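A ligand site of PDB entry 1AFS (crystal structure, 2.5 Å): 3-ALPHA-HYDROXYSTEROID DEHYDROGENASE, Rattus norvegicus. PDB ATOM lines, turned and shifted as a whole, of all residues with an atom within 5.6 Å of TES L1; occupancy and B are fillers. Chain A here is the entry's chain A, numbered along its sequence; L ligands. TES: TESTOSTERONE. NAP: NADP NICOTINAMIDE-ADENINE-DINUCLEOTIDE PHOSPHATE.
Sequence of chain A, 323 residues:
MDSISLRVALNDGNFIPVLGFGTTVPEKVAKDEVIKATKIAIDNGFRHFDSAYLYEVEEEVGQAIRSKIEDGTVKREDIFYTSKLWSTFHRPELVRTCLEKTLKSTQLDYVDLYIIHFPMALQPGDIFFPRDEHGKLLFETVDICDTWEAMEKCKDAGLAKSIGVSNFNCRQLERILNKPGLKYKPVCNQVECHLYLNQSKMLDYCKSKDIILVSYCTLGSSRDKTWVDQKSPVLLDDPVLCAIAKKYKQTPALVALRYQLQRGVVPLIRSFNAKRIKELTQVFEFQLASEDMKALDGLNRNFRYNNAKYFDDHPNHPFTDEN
OH of Tyr 55 is in hydrogen-bond range of O3 of TES L1, 2.6 Å away.
A ring nitrogen (NE2) of His 117 is in hydrogen-bond range of an oxygen (O3) of TES L1, 2.8 Å away.
An oxygen (O7N) of NAP L2 sits at hydrogen-bond distance from a ring nitrogen (NE2) of His 117.
An oxygen (O3D) of NAP L2 lies within hydrogen-bond range of the backbone NH of Thr 24 (3.3 Å).
The side-chain hydroxyl (OG1) of Thr 24 is in hydrogen-bond range of an oxygen (O3D) of NAP L2 (2.7 Å).
An oxygen (O7N) of NAP L2 lies within hydrogen-bond range of the side-chain amide nitrogen (ND2) of Asn 167 (2.8 Å).
Leu 54 touches TES L1 (CD2 to C1, 3.8 Å).
Phe 118 touches TES L1 (CE2 to C2, 3.96 Å).
Phe 129 touches TES L1.
Thr 226 touches TES L1.
Trp 227 touches TES L1 (NE1 to C6, 3.7 Å).
OD1 of Asn 306 touches C19 of TES L1, 3.9 Å away.
Tyr 310 touches TES L1 (OH to C19, 3.2 Å).
Hydrophobic or aromatic side chains within 4 Å of TES L1: Leu 54, Tyr 55, His 117, Phe 118, Phe 129, Trp 227 and Tyr 310.
The side-chain hydroxyl (OH) of Tyr 55 is in hydrogen-bond range of the side-chain amino group (NZ) of Lys 84 (3.0 Å).
The side-chain amide nitrogen (ND2) of Asn 167 lies within hydrogen-bond range of the backbone carbonyl oxygen (O) of His 117.
The side-chain amide oxygen of Asn 306 sits at hydrogen-bond distance from the side-chain hydroxyl of Tyr 310 (2.8 Å).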
ATOM      1  N   THR A  24      20.931  21.392 -28.564  1.00  0.00           N
ATOM      2  CA  THR A  24      20.674  22.518 -27.655  1.00  0.00           C
ATOM      3  C   THR A  24      21.330  22.240 -26.295  1.00  0.00           C
ATOM      4  O   THR A  24      21.303  21.115 -25.792  1.00  0.00           O
ATOM      5  CB  THR A  24      19.153  22.706 -27.419  1.00  0.00           C
ATOM      6  OG1 THR A  24      18.562  21.457 -27.060  1.00  0.00           O
ATOM      7  CG2 THR A  24      18.448  23.254 -28.653  1.00  0.00           C
ATOM      8  N   GLU A  27      20.268  25.752 -20.119  1.00  0.00           N
ATOM      9  CA  GLU A  27      20.709  27.007 -19.497  1.00  0.00           C
ATOM     10  C   GLU A  27      21.890  26.960 -18.536  1.00  0.00           C
ATOM     11  O   GLU A  27      22.834  27.748 -18.656  1.00  0.00           O
ATOM     12  CB  GLU A  27      19.521  27.716 -18.839  1.00  0.00           C
ATOM     13  CG  GLU A  27      19.713  29.230 -18.654  1.00  0.00           C
ATOM     14  CD  GLU A  27      19.955  29.986 -19.978  1.00  0.00           C
ATOM     15  OE1 GLU A  27      19.052  29.984 -20.855  1.00  0.00           O
ATOM     16  OE2 GLU A  27      21.047  30.570 -20.137  1.00  0.00           O
ATOM     17  N   ALA A  52      21.280  24.650 -34.959  1.00  0.00           N
ATOM     18  CA  ALA A  52      20.658  25.894 -35.405  1.00  0.00           C
ATOM     19  C   ALA A  52      21.548  27.085 -35.150  1.00  0.00           C
ATOM     20  O   ALA A  52      22.458  27.030 -34.320  1.00  0.00           O
ATOM     21  CB  ALA A  52      19.336  26.095 -34.701  1.00  0.00           C
ATOM     22  N   LEU A  54      20.480  29.907 -33.930  1.00  0.00           N
ATOM     23  CA  LEU A  54      20.038  30.356 -32.624  1.00  0.00           C
ATOM     24  C   LEU A  54      20.721  29.670 -31.432  1.00  0.00           C
ATOM     25  O   LEU A  54      20.962  30.311 -30.412  1.00  0.00           O
ATOM     26  CB  LEU A  54      18.528  30.149 -32.515  1.00  0.00           C
ATOM     27  CG  LEU A  54      17.901  30.549 -31.178  1.00  0.00           C
ATOM     28  CD1 LEU A  54      17.747  32.046 -31.139  1.00  0.00           C
ATOM     29  CD2 LEU A  54      16.541  29.872 -31.038  1.00  0.00           C
ATOM     30  N   TYR A  55      21.053  28.381 -31.557  1.00  0.00           N
ATOM     31  CA  TYR A  55      21.665  27.615 -30.459  1.00  0.00           C
ATOM     32  C   TYR A  55      23.049  28.070 -30.025  1.00  0.00           C
ATOM     33  O   TYR A  55      23.529  27.674 -28.960  1.00  0.00           O
ATOM     34  CB  TYR A  55      21.729  26.114 -30.796  1.00  0.00           C
ATOM     35  CG  TYR A  55      20.408  25.426 -31.083  1.00  0.00           C
ATOM     36  CD1 TYR A  55      19.191  26.107 -30.931  1.00  0.00           C
ATOM     37  CD2 TYR A  55      20.371  24.132 -31.587  1.00  0.00           C
ATOM     38  CE1 TYR A  55      17.971  25.509 -31.282  1.00  0.00           C
ATOM     39  CE2 TYR A  55      19.171  23.532 -31.960  1.00  0.00           C
ATOM     40  CZ  TYR A  55      17.978  24.230 -31.806  1.00  0.00           C
ATOM     41  OH  TYR A  55      16.799  23.686 -32.236  1.00  0.00           O
ATOM     42  N   LYS A  84      19.426  25.619 -38.955  1.00  0.00           N
ATOM     43  CA  LYS A  84      18.206  26.374 -39.195  1.00  0.00           C
ATOM     44  C   LYS A  84      18.437  27.868 -39.349  1.00  0.00           C
ATOM     45  O   LYS A  84      19.298  28.432 -38.683  1.00  0.00           O
ATOM     46  CB  LYS A  84      17.181  26.122 -38.075  1.00  0.00           C
ATOM     47  CG  LYS A  84      17.167  24.685 -37.528  1.00  0.00           C
ATOM     48  CD  LYS A  84      15.981  24.470 -36.629  1.00  0.00           C
ATOM     49  CE  LYS A  84      16.027  23.106 -35.993  1.00  0.00           C
ATOM     50  NZ  LYS A  84      17.209  22.938 -35.107  1.00  0.00           N
ATOM     51  N   TRP A  86      17.673  31.657 -38.864  1.00  0.00           N
ATOM     52  CA  TRP A  86      17.032  32.437 -37.825  1.00  0.00           C
ATOM     53  C   TRP A  86      16.121  33.547 -38.388  1.00  0.00           C
ATOM     54  O   TRP A  86      16.310  34.005 -39.514  1.00  0.00           O
ATOM     55  CB  TRP A  86      18.051  32.937 -36.801  1.00  0.00           C
ATOM     56  CG  TRP A  86      17.386  33.547 -35.623  1.00  0.00           C
ATOM     57  CD1 TRP A  86      17.551  34.820 -35.152  1.00  0.00           C
ATOM     58  CD2 TRP A  86      16.302  32.981 -34.859  1.00  0.00           C
ATOM     59  NE1 TRP A  86      16.617  35.079 -34.177  1.00  0.00           N
ATOM     60  CE2 TRP A  86      15.840  33.976 -33.973  1.00  0.00           C
ATOM     61  CE3 TRP A  86      15.670  31.727 -34.850  1.00  0.00           C
ATOM     62  CZ2 TRP A  86      14.787  33.764 -33.091  1.00  0.00           C
ATOM     63  CZ3 TRP A  86      14.615  31.502 -33.966  1.00  0.00           C
ATOM     64  CH2 TRP A  86      14.180  32.530 -33.103  1.00  0.00           C
ATOM     65  N   HIS A 117      13.578  28.010 -39.321  1.00  0.00           N
ATOM     66  CA  HIS A 117      13.271  27.730 -37.920  1.00  0.00           C
ATOM     67  C   HIS A 117      11.837  28.052 -37.473  1.00  0.00           C
ATOM     68  O   HIS A 117      11.224  27.258 -36.738  1.00  0.00           O
ATOM     69  CB  HIS A 117      14.285  28.450 -37.045  1.00  0.00           C
ATOM     70  CG  HIS A 117      14.508  27.800 -35.719  1.00  0.00           C
ATOM     71  ND1 HIS A 117      15.671  27.970 -34.991  1.00  0.00           N
ATOM     72  CD2 HIS A 117      13.717  26.989 -34.967  1.00  0.00           C
ATOM     73  CE1 HIS A 117      15.587  27.299 -33.856  1.00  0.00           C
ATOM     74  NE2 HIS A 117      14.408  26.706 -33.819  1.00  0.00           N
ATOM     75  N   PHE A 118      11.307  29.200 -37.898  1.00  0.00           N
ATOM     76  CA  PHE A 118       9.946  29.631 -37.551  1.00  0.00           C
ATOM     77  C   PHE A 118       9.421  30.426 -38.727  1.00  0.00           C
ATOM     78  O   PHE A 118      10.200  31.091 -39.418  1.00  0.00           O
ATOM     79  CB  PHE A 118       9.972  30.577 -36.342  1.00  0.00           C
ATOM     80  CG  PHE A 118      10.052  29.885 -35.011  1.00  0.00           C
ATOM     81  CD1 PHE A 118       8.910  29.394 -34.397  1.00  0.00           C
ATOM     82  CD2 PHE A 118      11.275  29.739 -34.379  1.00  0.00           C
ATOM     83  CE1 PHE A 118       8.976  28.783 -33.148  1.00  0.00           C
ATOM     84  CE2 PHE A 118      11.348  29.112 -33.127  1.00  0.00           C
ATOM     85  CZ  PHE A 118      10.201  28.645 -32.510  1.00  0.00           C
ATOM     86  N   PHE A 129      16.132  38.333 -30.640  1.00  0.00           N
ATOM     87  CA  PHE A 129      14.784  38.838 -30.448  1.00  0.00           C
ATOM     88  C   PHE A 129      14.831  40.340 -30.192  1.00  0.00           C
ATOM     89  O   PHE A 129      14.808  40.798 -29.056  1.00  0.00           O
ATOM     90  CB  PHE A 129      14.122  38.144 -29.252  1.00  0.00           C
ATOM     91  CG  PHE A 129      13.750  36.703 -29.520  1.00  0.00           C
ATOM     92  CD1 PHE A 129      14.643  35.678 -29.249  1.00  0.00           C
ATOM     93  CD2 PHE A 129      12.477  36.382 -29.976  1.00  0.00           C
ATOM     94  CE1 PHE A 129      14.266  34.346 -29.438  1.00  0.00           C
ATOM     95  CE2 PHE A 129      12.103  35.062 -30.168  1.00  0.00           C
ATOM     96  CZ  PHE A 129      12.998  34.046 -29.892  1.00  0.00           C
ATOM     97  N   ASN A 167       8.131  24.298 -37.407  1.00  0.00           N
ATOM     98  CA  ASN A 167       7.064  25.043 -36.735  1.00  0.00           C
ATOM     99  C   ASN A 167       6.037  25.725 -37.662  1.00  0.00           C
ATOM    100  O   ASN A 167       5.481  26.770 -37.324  1.00  0.00           O
ATOM    101  CB  ASN A 167       7.663  26.052 -35.740  1.00  0.00           C
ATOM    102  CG  ASN A 167       8.512  25.383 -34.672  1.00  0.00           C
ATOM    103  OD1 ASN A 167       8.059  24.445 -34.019  1.00  0.00           O
ATOM    104  ND2 ASN A 167       9.747  25.840 -34.503  1.00  0.00           N
ATOM    105  N   THR A 226      13.653  28.228 -18.615  1.00  0.00           N
ATOM    106  CA  THR A 226      13.669  29.467 -19.380  1.00  0.00           C
ATOM    107  C   THR A 226      12.603  29.405 -20.479  1.00  0.00           C
ATOM    108  O   THR A 226      12.179  30.441 -20.996  1.00  0.00           O
ATOM    109  CB  THR A 226      15.038  29.789 -20.026  1.00  0.00           C
ATOM    110  OG1 THR A 226      15.270  28.931 -21.149  1.00  0.00           O
ATOM    111  CG2 THR A 226      16.143  29.624 -19.004  1.00  0.00           C
ATOM    112  N   TRP A 227      12.167  28.189 -20.827  1.00  0.00           N
ATOM    113  CA  TRP A 227      11.142  28.069 -21.851  1.00  0.00           C
ATOM    114  C   TRP A 227      10.055  27.002 -21.625  1.00  0.00           C
ATOM    115  O   TRP A 227       9.066  26.963 -22.358  1.00  0.00           O
ATOM    116  CB  TRP A 227      11.759  27.951 -23.262  1.00  0.00           C
ATOM    117  CG  TRP A 227      12.498  26.705 -23.491  1.00  0.00           C
ATOM    118  CD1 TRP A 227      13.792  26.453 -23.153  1.00  0.00           C
ATOM    119  CD2 TRP A 227      12.001  25.522 -24.109  1.00  0.00           C
ATOM    120  NE1 TRP A 227      14.130  25.168 -23.512  1.00  0.00           N
ATOM    121  CE2 TRP A 227      13.048  24.573 -24.104  1.00  0.00           C
ATOM    122  CE3 TRP A 227      10.758  25.163 -24.668  1.00  0.00           C
ATOM    123  CZ2 TRP A 227      12.900  23.289 -24.639  1.00  0.00           C
ATOM    124  CZ3 TRP A 227      10.612  23.887 -25.197  1.00  0.00           C
ATOM    125  CH2 TRP A 227      11.676  22.966 -25.185  1.00  0.00           C
ATOM    126  N   ASN A 306       6.204  23.751 -26.011  1.00  0.00           N
ATOM    127  CA  ASN A 306       6.760  24.885 -26.779  1.00  0.00           C
ATOM    128  C   ASN A 306       5.655  25.738 -27.418  1.00  0.00           C
ATOM    129  O   ASN A 306       5.236  25.496 -28.554  1.00  0.00           O
ATOM    130  CB  ASN A 306       7.735  24.410 -27.849  1.00  0.00           C
ATOM    131  CG  ASN A 306       8.492  25.558 -28.489  1.00  0.00           C
ATOM    132  OD1 ASN A 306       8.716  26.580 -27.861  1.00  0.00           O
ATOM    133  ND2 ASN A 306       8.888  25.400 -29.738  1.00  0.00           N
ATOM    134  N   TYR A 310       7.611  33.663 -26.829  1.00  0.00           N
ATOM    135  CA  TYR A 310       8.722  34.602 -26.942  1.00  0.00           C
ATOM    136  C   TYR A 310       8.591  35.343 -28.272  1.00  0.00           C
ATOM    137  O   TYR A 310       9.387  36.222 -28.590  1.00  0.00           O
ATOM    138  CB  TYR A 310      10.084  33.898 -26.832  1.00  0.00           C
ATOM    139  CG  TYR A 310      10.144  32.497 -27.414  1.00  0.00           C
ATOM    140  CD1 TYR A 310      10.415  32.296 -28.775  1.00  0.00           C
ATOM    141  CD2 TYR A 310       9.867  31.372 -26.632  1.00  0.00           C
ATOM    142  CE1 TYR A 310      10.390  31.017 -29.326  1.00  0.00           C
ATOM    143  CE2 TYR A 310       9.851  30.086 -27.175  1.00  0.00           C
ATOM    144  CZ  TYR A 310      10.112  29.927 -28.523  1.00  0.00           C
ATOM    145  OH  TYR A 310      10.064  28.682 -29.080  1.00  0.00           O
HETATM  146  C1  TES L   1      13.531  27.988 -29.782  1.00  0.00           C
HETATM  147  C2  TES L   1      13.301  26.737 -30.636  1.00  0.00           C
HETATM  148  C3  TES L   1      14.446  25.802 -30.541  1.00  0.00           C
HETATM  149  O3  TES L   1      14.913  25.248 -31.507  1.00  0.00           O
HETATM  150  C4  TES L   1      14.982  25.588 -29.214  1.00  0.00           C
HETATM  151  C5  TES L   1      14.746  26.433 -28.182  1.00  0.00           C
HETATM  152  C6  TES L   1      15.383  26.162 -26.843  1.00  0.00           C
HETATM  153  C7  TES L   1      16.072  27.382 -26.261  1.00  0.00           C
HETATM  154  C8  TES L   1      15.087  28.560 -26.247  1.00  0.00           C
HETATM  155  C9  TES L   1      14.528  28.866 -27.649  1.00  0.00           C
HETATM  156  C10 TES L   1      13.823  27.670 -28.300  1.00  0.00           C
HETATM  157  C11 TES L   1      13.592  30.090 -27.742  1.00  0.00           C
HETATM  158  C12 TES L   1      14.265  31.329 -27.127  1.00  0.00           C
HETATM  159  C13 TES L   1      14.726  31.042 -25.700  1.00  0.00           C
HETATM  160  C14 TES L   1      15.688  29.851 -25.703  1.00  0.00           C
HETATM  161  C15 TES L   1      16.313  29.839 -24.310  1.00  0.00           C
HETATM  162  C16 TES L   1      16.483  31.335 -23.996  1.00  0.00           C
HETATM  163  C17 TES L   1      15.754  32.087 -25.141  1.00  0.00           C
HETATM  164  O17 TES L   1      15.187  33.350 -24.739  1.00  0.00           O
HETATM  165  C18 TES L   1      13.543  30.834 -24.737  1.00  0.00           C
HETATM  166  C19 TES L   1      12.514  27.337 -27.548  1.00  0.00           C
HETATM  167  PA  NAP L   2      13.588  15.937 -25.590  1.00  0.00           P
HETATM  168  O1A NAP L   2      12.152  15.575 -25.606  1.00  0.00           O
HETATM  169  O2A NAP L   2      14.493  15.228 -26.519  1.00  0.00           O
HETATM  170  O5B NAP L   2      14.111  15.690 -24.096  1.00  0.00           O
HETATM  171  C5B NAP L   2      15.508  15.761 -23.770  1.00  0.00           C
HETATM  172  C4B NAP L   2      15.554  15.226 -22.369  1.00  0.00           C
HETATM  173  O4B NAP L   2      15.247  13.822 -22.380  1.00  0.00           O
HETATM  174  C3B NAP L   2      16.942  15.413 -21.805  1.00  0.00           C
HETATM  175  O3B NAP L   2      16.839  16.193 -20.608  1.00  0.00           O
HETATM  176  C2B NAP L   2      17.463  14.012 -21.529  1.00  0.00           C
HETATM  177  O2B NAP L   2      18.093  13.940 -20.232  1.00  0.00           O
HETATM  178  C1B NAP L   2      16.213  13.152 -21.560  1.00  0.00           C
HETATM  179  N9A NAP L   2      16.507  11.783 -22.072  1.00  0.00           N
HETATM  180  C8A NAP L   2      17.217  11.453 -23.154  1.00  0.00           C
HETATM  181  N7A NAP L   2      17.306  10.128 -23.247  1.00  0.00           N
HETATM  182  C5A NAP L   2      16.638   9.606 -22.218  1.00  0.00           C
HETATM  183  C6A NAP L   2      16.356   8.312 -21.791  1.00  0.00           C
HETATM  184  N6A NAP L   2      16.729   7.217 -22.454  1.00  0.00           N
HETATM  185  N1A NAP L   2      15.615   8.138 -20.672  1.00  0.00           N
HETATM  186  C2A NAP L   2      15.167   9.173 -19.983  1.00  0.00           C
HETATM  187  N3A NAP L   2      15.419  10.418 -20.361  1.00  0.00           N
HETATM  188  C4A NAP L   2      16.135  10.661 -21.465  1.00  0.00           C
HETATM  189  O3  NAP L   2      13.678  17.539 -25.765  1.00  0.00           O
HETATM  190  PN  NAP L   2      14.734  18.737 -25.937  1.00  0.00           P
HETATM  191  O1N NAP L   2      16.042  18.382 -25.353  1.00  0.00           O
HETATM  192  O2N NAP L   2      14.070  19.972 -25.457  1.00  0.00           O
HETATM  193  O5D NAP L   2      14.865  18.846 -27.535  1.00  0.00           O
HETATM  194  C5D NAP L   2      15.654  17.925 -28.301  1.00  0.00           C
HETATM  195  C4D NAP L   2      16.037  18.536 -29.640  1.00  0.00           C
HETATM  196  O4D NAP L   2      14.904  18.871 -30.464  1.00  0.00           O
HETATM  197  C3D NAP L   2      16.787  19.841 -29.472  1.00  0.00           C
HETATM  198  O3D NAP L   2      18.162  19.674 -29.108  1.00  0.00           O
HETATM  199  C2D NAP L   2      16.680  20.421 -30.864  1.00  0.00           C
HETATM  200  O2D NAP L   2      17.719  19.886 -31.680  1.00  0.00           O
HETATM  201  C1D NAP L   2      15.300  19.988 -31.296  1.00  0.00           C
HETATM  202  N1N NAP L   2      14.345  21.095 -31.073  1.00  0.00           N
HETATM  203  C2N NAP L   2      13.912  21.878 -32.151  1.00  0.00           C
HETATM  204  C3N NAP L   2      13.003  22.915 -31.930  1.00  0.00           C
HETATM  205  C7N NAP L   2      12.473  23.735 -33.104  1.00  0.00           C
HETATM  206  O7N NAP L   2      11.817  24.760 -32.920  1.00  0.00           O
HETATM  207  N7N NAP L   2      12.760  23.270 -34.308  1.00  0.00           N
HETATM  208  C4N NAP L   2      12.548  23.176 -30.649  1.00  0.00           C
HETATM  209  C5N NAP L   2      12.985  22.406 -29.573  1.00  0.00           C
HETATM  210  C6N NAP L   2      13.873  21.368 -29.785  1.00  0.00           C
HETATM  211  P2B NAP L   2      19.650  13.599 -20.061  1.00  0.00           P
HETATM  212  O1X NAP L   2      20.451  14.552 -20.865  1.00  0.00           O
HETATM  213  O2X NAP L   2      19.927  13.492 -18.615  1.00  0.00           O
HETATM  214  O3X NAP L   2      19.787  12.137 -20.708  1.00  0.00           O
